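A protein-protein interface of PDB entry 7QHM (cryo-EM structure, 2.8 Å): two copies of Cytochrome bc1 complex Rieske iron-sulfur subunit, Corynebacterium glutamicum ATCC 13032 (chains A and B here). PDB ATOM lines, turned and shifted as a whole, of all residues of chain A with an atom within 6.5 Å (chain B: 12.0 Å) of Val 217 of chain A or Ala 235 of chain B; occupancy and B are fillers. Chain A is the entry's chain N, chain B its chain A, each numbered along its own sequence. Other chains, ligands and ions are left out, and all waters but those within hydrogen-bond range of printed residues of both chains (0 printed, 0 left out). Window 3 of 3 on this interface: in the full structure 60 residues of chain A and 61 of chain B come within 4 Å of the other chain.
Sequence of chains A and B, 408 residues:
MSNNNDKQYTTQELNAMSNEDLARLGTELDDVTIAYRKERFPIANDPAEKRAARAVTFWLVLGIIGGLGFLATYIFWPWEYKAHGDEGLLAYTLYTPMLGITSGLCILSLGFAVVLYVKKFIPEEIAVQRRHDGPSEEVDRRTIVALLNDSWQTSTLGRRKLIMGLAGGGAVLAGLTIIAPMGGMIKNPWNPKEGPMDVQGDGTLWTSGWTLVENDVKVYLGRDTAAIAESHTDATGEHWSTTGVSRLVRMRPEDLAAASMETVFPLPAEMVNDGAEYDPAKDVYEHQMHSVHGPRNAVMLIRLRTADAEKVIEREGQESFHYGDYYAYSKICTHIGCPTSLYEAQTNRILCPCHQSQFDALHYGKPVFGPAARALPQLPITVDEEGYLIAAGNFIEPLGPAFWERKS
The side-chain carboxylate (OD1) of Asp 234 of chain B is in hydrogen-bond range of the side-chain hydroxyl (OG1) of Thr 236 of chain B, at 2.5 Å.
A ring nitrogen (NE2) of His 239 of chain B lies within hydrogen-bond range of the side-chain hydroxyl (OG1) of Thr 236 of chain B (3.5 Å).
A ring nitrogen (NE2) of His 239 of chain B is in hydrogen-bond range of the backbone carbonyl oxygen (O) of Gly 237 of chain B.
Among the printed residues, pairs that only touch across the chains: Met 197 of chain A with Thr 236 of chain B, Met 197 of chain A with Gly 237 of chain B, Asp 198 of chain A with Thr 236 of chain B, Leu 212 of chain A with Ala 235 of chain B, Val 217 of chain A with Ala 235 of chain B, Pro 268 of chain A with Thr 236 of chain B and Glu 270 of chain A with Thr 236 of chain B.
Of the printed residues of chain B, Met 197 of chain A touches Thr 236 (3.7 Å) and Gly 237 (3.7 Å).
Of the printed residues of chain B, Asp 198 of chain A touches Thr 236.
Leu 212 of chain A touches just one residue of chain B: Ala 235 (3.9 Å).
No residue of chain B comes within 4 Å of Val 213 of chain A.
No residue of chain B comes within 4 Å of Asp 216 of chain A.
Of the printed residues of chain B, Val 217 of chain A touches Ala 235 (3.9 Å).
Pro 268 of chain A touches one residue of chain B.
Of the printed residues of chain B, Glu 270 of chain A touches Thr 236 (3.98 Å).
Ala 391 of chain A touches none of the printed residues of chain B.
Ala 235 of chain B touches just these residues of chain A: Leu 212 (3.9 Å) and Val 217 (3.9 Å).
Of the printed residues of chain A, Thr 236 of chain B touches Met 197 (3.7 Å), Asp 198 (3.5 Å), Pro 268 (3.6 Å) and Glu 270 (3.98 Å).
Printed residues of chain A within 4 Å of Gly 237 of chain B: Met 197 (3.7 Å).
The nearest residue of chain B that does not touch Val 217 of chain A is Thr 236 of chain B (4.5 Å).
The nearest residue of chain A that does not touch Ala 235 of chain B is Met 197 of chain A (4.3 Å).
Of the 9 printed residues of chain B, 3 touch a printed residue of chain A.
Printed residues of chain B that touch a printed residue of chain A: Ala 235, Thr 236 and Gly 237.
Hydrophobic or aromatic side chains of chain B that line the printed part of chain A: Ala 235.
Along chain B the printed residues that touch a printed residue of chain A span positions 235 to 237.
Hydrophobic or aromatic side chains of chain A within 4 Å of the printed part of chain B: Leu 212, Val 217 and Pro 268.
Among the printed residues, 7 pairs touch across the chains.
No position is printed for both chains.
Of the 7 pairs that touch across the chains among the printed residues, none has its exchanged pair printed and touching as well.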
ATOM      1  N   MET A 197      20.502   2.348  -6.365  1.00  0.00           N
ATOM      2  CA  MET A 197      20.510   3.560  -7.169  1.00  0.00           C
ATOM      3  C   MET A 197      19.104   3.883  -7.651  1.00  0.00           C
ATOM      4  O   MET A 197      18.358   2.998  -8.073  1.00  0.00           O
ATOM      5  CB  MET A 197      21.463   3.377  -8.346  1.00  0.00           C
ATOM      6  CG  MET A 197      21.580   4.557  -9.285  1.00  0.00           C
ATOM      7  SD  MET A 197      22.703   4.215 -10.640  1.00  0.00           S
ATOM      8  CE  MET A 197      24.283   4.355  -9.812  1.00  0.00           C
ATOM      9  N   ASP A 198      18.748   5.165  -7.588  1.00  0.00           N
ATOM     10  CA  ASP A 198      17.413   5.659  -7.892  1.00  0.00           C
ATOM     11  C   ASP A 198      17.490   6.699  -9.009  1.00  0.00           C
ATOM     12  O   ASP A 198      18.502   6.828  -9.700  1.00  0.00           O
ATOM     13  CB  ASP A 198      16.755   6.201  -6.621  1.00  0.00           C
ATOM     14  CG  ASP A 198      17.490   7.388  -6.022  1.00  0.00           C
ATOM     15  OD1 ASP A 198      18.491   7.860  -6.588  1.00  0.00           O
ATOM     16  OD2 ASP A 198      17.063   7.849  -4.945  1.00  0.00           O
ATOM     17  N   LEU A 212      20.745   5.011 -14.639  1.00  0.00           N
ATOM     18  CA  LEU A 212      19.926   3.809 -14.613  1.00  0.00           C
ATOM     19  C   LEU A 212      19.923   3.076 -15.942  1.00  0.00           C
ATOM     20  O   LEU A 212      19.676   1.868 -15.959  1.00  0.00           O
ATOM     21  CB  LEU A 212      18.491   4.164 -14.228  1.00  0.00           C
ATOM     22  CG  LEU A 212      18.267   4.606 -12.783  1.00  0.00           C
ATOM     23  CD1 LEU A 212      16.889   5.194 -12.614  1.00  0.00           C
ATOM     24  CD2 LEU A 212      18.459   3.455 -11.826  1.00  0.00           C
ATOM     25  N   VAL A 213      20.189   3.767 -17.051  1.00  0.00           N
ATOM     26  CA  VAL A 213      20.236   3.094 -18.344  1.00  0.00           C
ATOM     27  C   VAL A 213      21.307   2.018 -18.336  1.00  0.00           C
ATOM     28  O   VAL A 213      21.119   0.933 -18.894  1.00  0.00           O
ATOM     29  CB  VAL A 213      20.466   4.110 -19.479  1.00  0.00           C
ATOM     30  CG1 VAL A 213      20.558   3.397 -20.810  1.00  0.00           C
ATOM     31  CG2 VAL A 213      19.342   5.123 -19.521  1.00  0.00           C
ATOM     32  N   GLU A 214      22.435   2.284 -17.676  1.00  0.00           N
ATOM     33  CA  GLU A 214      23.509   1.300 -17.608  1.00  0.00           C
ATOM     34  C   GLU A 214      23.164   0.096 -16.739  1.00  0.00           C
ATOM     35  O   GLU A 214      23.903  -0.890 -16.776  1.00  0.00           O
ATOM     36  CB  GLU A 214      24.787   1.962 -17.095  1.00  0.00           C
ATOM     37  CG  GLU A 214      25.293   3.116 -17.960  1.00  0.00           C
ATOM     38  CD  GLU A 214      25.728   2.684 -19.359  1.00  0.00           C
ATOM     39  OE1 GLU A 214      26.200   1.537 -19.514  1.00  0.00           O
ATOM     40  OE2 GLU A 214      25.594   3.491 -20.306  1.00  0.00           O
ATOM     41  N   ASN A 215      22.084   0.151 -15.957  1.00  0.00           N
ATOM     42  CA  ASN A 215      21.555  -1.004 -15.238  1.00  0.00           C
ATOM     43  C   ASN A 215      20.510  -1.770 -16.045  1.00  0.00           C
ATOM     44  O   ASN A 215      19.784  -2.590 -15.475  1.00  0.00           O
ATOM     45  CB  ASN A 215      20.936  -0.567 -13.912  1.00  0.00           C
ATOM     46  CG  ASN A 215      21.905   0.177 -13.036  1.00  0.00           C
ATOM     47  OD1 ASN A 215      22.991   0.550 -13.473  1.00  0.00           O
ATOM     48  ND2 ASN A 215      21.514   0.416 -11.792  1.00  0.00           N
ATOM     49  N   ASP A 216      20.409  -1.515 -17.349  1.00  0.00           N
ATOM     50  CA  ASP A 216      19.438  -2.181 -18.210  1.00  0.00           C
ATOM     51  C   ASP A 216      18.009  -1.897 -17.747  1.00  0.00           C
ATOM     52  O   ASP A 216      17.175  -2.794 -17.619  1.00  0.00           O
ATOM     53  CB  ASP A 216      19.712  -3.684 -18.279  1.00  0.00           C
ATOM     54  CG  ASP A 216      18.951  -4.366 -19.395  1.00  0.00           C
ATOM     55  OD1 ASP A 216      18.286  -3.665 -20.188  1.00  0.00           O
ATOM     56  OD2 ASP A 216      19.013  -5.609 -19.477  1.00  0.00           O
ATOM     57  N   VAL A 217      17.740  -0.627 -17.477  1.00  0.00           N
ATOM     58  CA  VAL A 217      16.395  -0.114 -17.255  1.00  0.00           C
ATOM     59  C   VAL A 217      16.020   0.677 -18.496  1.00  0.00           C
ATOM     60  O   VAL A 217      16.855   1.396 -19.051  1.00  0.00           O
ATOM     61  CB  VAL A 217      16.327   0.772 -15.991  1.00  0.00           C
ATOM     62  CG1 VAL A 217      14.927   1.299 -15.772  1.00  0.00           C
ATOM     63  CG2 VAL A 217      16.779   0.011 -14.765  1.00  0.00           C
ATOM     64  N   LYS A 218      14.778   0.541 -18.946  1.00  0.00           N
ATOM     65  CA  LYS A 218      14.284   1.437 -19.981  1.00  0.00           C
ATOM     66  C   LYS A 218      13.912   2.757 -19.321  1.00  0.00           C
ATOM     67  O   LYS A 218      13.095   2.785 -18.397  1.00  0.00           O
ATOM     68  CB  LYS A 218      13.088   0.854 -20.731  1.00  0.00           C
ATOM     69  CG  LYS A 218      12.732   1.661 -21.977  1.00  0.00           C
ATOM     70  CD  LYS A 218      11.421   1.271 -22.597  1.00  0.00           C
ATOM     71  CE  LYS A 218      11.566   0.173 -23.624  1.00  0.00           C
ATOM     72  NZ  LYS A 218      10.288  -0.036 -24.356  1.00  0.00           N
ATOM     73  N   VAL A 219      14.521   3.838 -19.794  1.00  0.00           N
ATOM     74  CA  VAL A 219      14.302   5.177 -19.274  1.00  0.00           C
ATOM     75  C   VAL A 219      13.790   6.017 -20.429  1.00  0.00           C
ATOM     76  O   VAL A 219      14.560   6.388 -21.321  1.00  0.00           O
ATOM     77  CB  VAL A 219      15.579   5.781 -18.677  1.00  0.00           C
ATOM     78  CG1 VAL A 219      15.309   7.171 -18.126  1.00  0.00           C
ATOM     79  CG2 VAL A 219      16.120   4.895 -17.588  1.00  0.00           C
ATOM     80  N   PRO A 268      11.720   6.300 -15.739  1.00  0.00           N
ATOM     81  CA  PRO A 268      11.798   4.847 -15.873  1.00  0.00           C
ATOM     82  C   PRO A 268      10.441   4.238 -16.177  1.00  0.00           C
ATOM     83  O   PRO A 268       9.393   4.796 -15.858  1.00  0.00           O
ATOM     84  CB  PRO A 268      12.320   4.394 -14.508  1.00  0.00           C
ATOM     85  CG  PRO A 268      13.043   5.544 -13.993  1.00  0.00           C
ATOM     86  CD  PRO A 268      12.313   6.745 -14.471  1.00  0.00           C
ATOM     87  N   ALA A 269      10.480   3.059 -16.801  1.00  0.00           N
ATOM     88  CA  ALA A 269       9.261   2.401 -17.251  1.00  0.00           C
ATOM     89  C   ALA A 269       8.327   2.049 -16.105  1.00  0.00           C
ATOM     90  O   ALA A 269       7.124   1.896 -16.328  1.00  0.00           O
ATOM     91  CB  ALA A 269       9.614   1.143 -18.036  1.00  0.00           C
ATOM     92  N   GLU A 270       8.845   1.926 -14.888  1.00  0.00           N
ATOM     93  CA  GLU A 270       8.042   1.554 -13.733  1.00  0.00           C
ATOM     94  C   GLU A 270       7.265   2.720 -13.137  1.00  0.00           C
ATOM     95  O   GLU A 270       6.553   2.519 -12.151  1.00  0.00           O
ATOM     96  CB  GLU A 270       8.945   0.938 -12.661  1.00  0.00           C
ATOM     97  CG  GLU A 270       9.271  -0.535 -12.893  1.00  0.00           C
ATOM     98  CD  GLU A 270      10.040  -0.774 -14.173  1.00  0.00           C
ATOM     99  OE1 GLU A 270      10.818   0.116 -14.568  1.00  0.00           O
ATOM    100  OE2 GLU A 270       9.853  -1.840 -14.794  1.00  0.00           O
ATOM    101  N   ALA A 391      16.347   7.015 -23.840  1.00  0.00           N
ATOM    102  CA  ALA A 391      17.776   7.287 -23.750  1.00  0.00           C
ATOM    103  C   ALA A 391      18.533   6.017 -24.102  1.00  0.00           C
ATOM    104  O   ALA A 391      18.491   5.038 -23.354  1.00  0.00           O
ATOM    105  CB  ALA A 391      18.145   7.763 -22.351  1.00  0.00           C
ATOM    106  N   SER B 231       8.724  -1.886   2.628  1.00  0.00           N
ATOM    107  CA  SER B 231       9.819  -1.482   1.753  1.00  0.00           C
ATOM    108  C   SER B 231       9.811  -2.368   0.511  1.00  0.00           C
ATOM    109  O   SER B 231      10.395  -3.448   0.480  1.00  0.00           O
ATOM    110  CB  SER B 231      11.141  -1.552   2.503  1.00  0.00           C
ATOM    111  OG  SER B 231      12.081  -0.668   1.933  1.00  0.00           O
ATOM    112  N   HIS B 232       9.117  -1.906  -0.522  1.00  0.00           N
ATOM    113  CA  HIS B 232       9.219  -2.509  -1.839  1.00  0.00           C
ATOM    114  C   HIS B 232      10.565  -2.138  -2.456  1.00  0.00           C
ATOM    115  O   HIS B 232      11.157  -1.116  -2.118  1.00  0.00           O
ATOM    116  CB  HIS B 232       8.046  -2.029  -2.701  1.00  0.00           C
ATOM    117  CG  HIS B 232       8.216  -2.268  -4.167  1.00  0.00           C
ATOM    118  ND1 HIS B 232       8.405  -3.523  -4.702  1.00  0.00           N
ATOM    119  CD2 HIS B 232       8.227  -1.407  -5.213  1.00  0.00           C
ATOM    120  CE1 HIS B 232       8.528  -3.425  -6.015  1.00  0.00           C
ATOM    121  NE2 HIS B 232       8.422  -2.152  -6.349  1.00  0.00           N
ATOM    122  N   THR B 233      11.076  -2.995  -3.336  1.00  0.00           N
ATOM    123  CA  THR B 233      12.359  -2.737  -3.978  1.00  0.00           C
ATOM    124  C   THR B 233      12.325  -3.262  -5.402  1.00  0.00           C
ATOM    125  O   THR B 233      11.847  -4.372  -5.649  1.00  0.00           O
ATOM    126  CB  THR B 233      13.507  -3.388  -3.206  1.00  0.00           C
ATOM    127  OG1 THR B 233      13.515  -2.891  -1.864  1.00  0.00           O
ATOM    128  CG2 THR B 233      14.846  -3.077  -3.853  1.00  0.00           C
ATOM    129  N   ASP B 234      12.843  -2.462  -6.330  1.00  0.00           N
ATOM    130  CA  ASP B 234      12.863  -2.817  -7.742  1.00  0.00           C
ATOM    131  C   ASP B 234      14.046  -2.124  -8.402  1.00  0.00           C
ATOM    132  O   ASP B 234      14.854  -1.467  -7.739  1.00  0.00           O
ATOM    133  CB  ASP B 234      11.531  -2.451  -8.405  1.00  0.00           C
ATOM    134  CG  ASP B 234      11.158  -1.000  -8.202  1.00  0.00           C
ATOM    135  OD1 ASP B 234      11.916  -0.112  -8.634  1.00  0.00           O
ATOM    136  OD2 ASP B 234      10.087  -0.744  -7.616  1.00  0.00           O
ATOM    137  N   ALA B 235      14.134  -2.259  -9.727  1.00  0.00           N
ATOM    138  CA  ALA B 235      15.262  -1.751 -10.498  1.00  0.00           C
ATOM    139  C   ALA B 235      15.423  -0.237 -10.424  1.00  0.00           C
ATOM    140  O   ALA B 235      16.479   0.266 -10.814  1.00  0.00           O
ATOM    141  CB  ALA B 235      15.107  -2.176 -11.958  1.00  0.00           C
ATOM    142  N   THR B 236      14.419   0.493  -9.948  1.00  0.00           N
ATOM    143  CA  THR B 236      14.469   1.943  -9.838  1.00  0.00           C
ATOM    144  C   THR B 236      14.688   2.429  -8.411  1.00  0.00           C
ATOM    145  O   THR B 236      14.574   3.631  -8.164  1.00  0.00           O
ATOM    146  CB  THR B 236      13.182   2.554 -10.379  1.00  0.00           C
ATOM    147  OG1 THR B 236      12.093   2.193  -9.524  1.00  0.00           O
ATOM    148  CG2 THR B 236      12.891   2.060 -11.784  1.00  0.00           C
ATOM    149  N   GLY B 237      14.971   1.532  -7.463  1.00  0.00           N
ATOM    150  CA  GLY B 237      15.334   1.896  -6.111  1.00  0.00           C
ATOM    151  C   GLY B 237      14.535   1.127  -5.087  1.00  0.00           C
ATOM    152  O   GLY B 237      13.900   0.112  -5.386  1.00  0.00           O
ATOM    153  N   GLU B 238      14.586   1.615  -3.851  1.00  0.00           N
ATOM    154  CA  GLU B 238      13.868   1.045  -2.721  1.00  0.00           C
ATOM    155  C   GLU B 238      12.909   2.090  -2.176  1.00  0.00           C
ATOM    156  O   GLU B 238      13.307   3.231  -1.927  1.00  0.00           O
ATOM    157  CB  GLU B 238      14.830   0.592  -1.629  1.00  0.00           C
ATOM    158  CG  GLU B 238      14.147   0.111  -0.373  1.00  0.00           C
ATOM    159  CD  GLU B 238      15.055  -0.733   0.488  1.00  0.00           C
ATOM    160  OE1 GLU B 238      16.196  -0.300   0.758  1.00  0.00           O
ATOM    161  OE2 GLU B 238      14.632  -1.837   0.891  1.00  0.00           O
ATOM    162  N   HIS B 239      11.654   1.693  -1.985  1.00  0.00           N
ATOM    163  CA  HIS B 239      10.554   2.612  -1.740  1.00  0.00           C
ATOM    164  C   HIS B 239       9.723   2.090  -0.580  1.00  0.00           C
ATOM    165  O   HIS B 239       9.164   0.994  -0.666  1.00  0.00           O
ATOM    166  CB  HIS B 239       9.687   2.748  -2.992  1.00  0.00           C
ATOM    167  CG  HIS B 239      10.439   2.556  -4.272  1.00  0.00           C
ATOM    168  ND1 HIS B 239      11.175   3.560  -4.862  1.00  0.00           N
ATOM    169  CD2 HIS B 239      10.570   1.474  -5.075  1.00  0.00           C
ATOM    170  CE1 HIS B 239      11.723   3.106  -5.974  1.00  0.00           C
ATOM    171  NE2 HIS B 239      11.371   1.844  -6.127  1.00  0.00           N
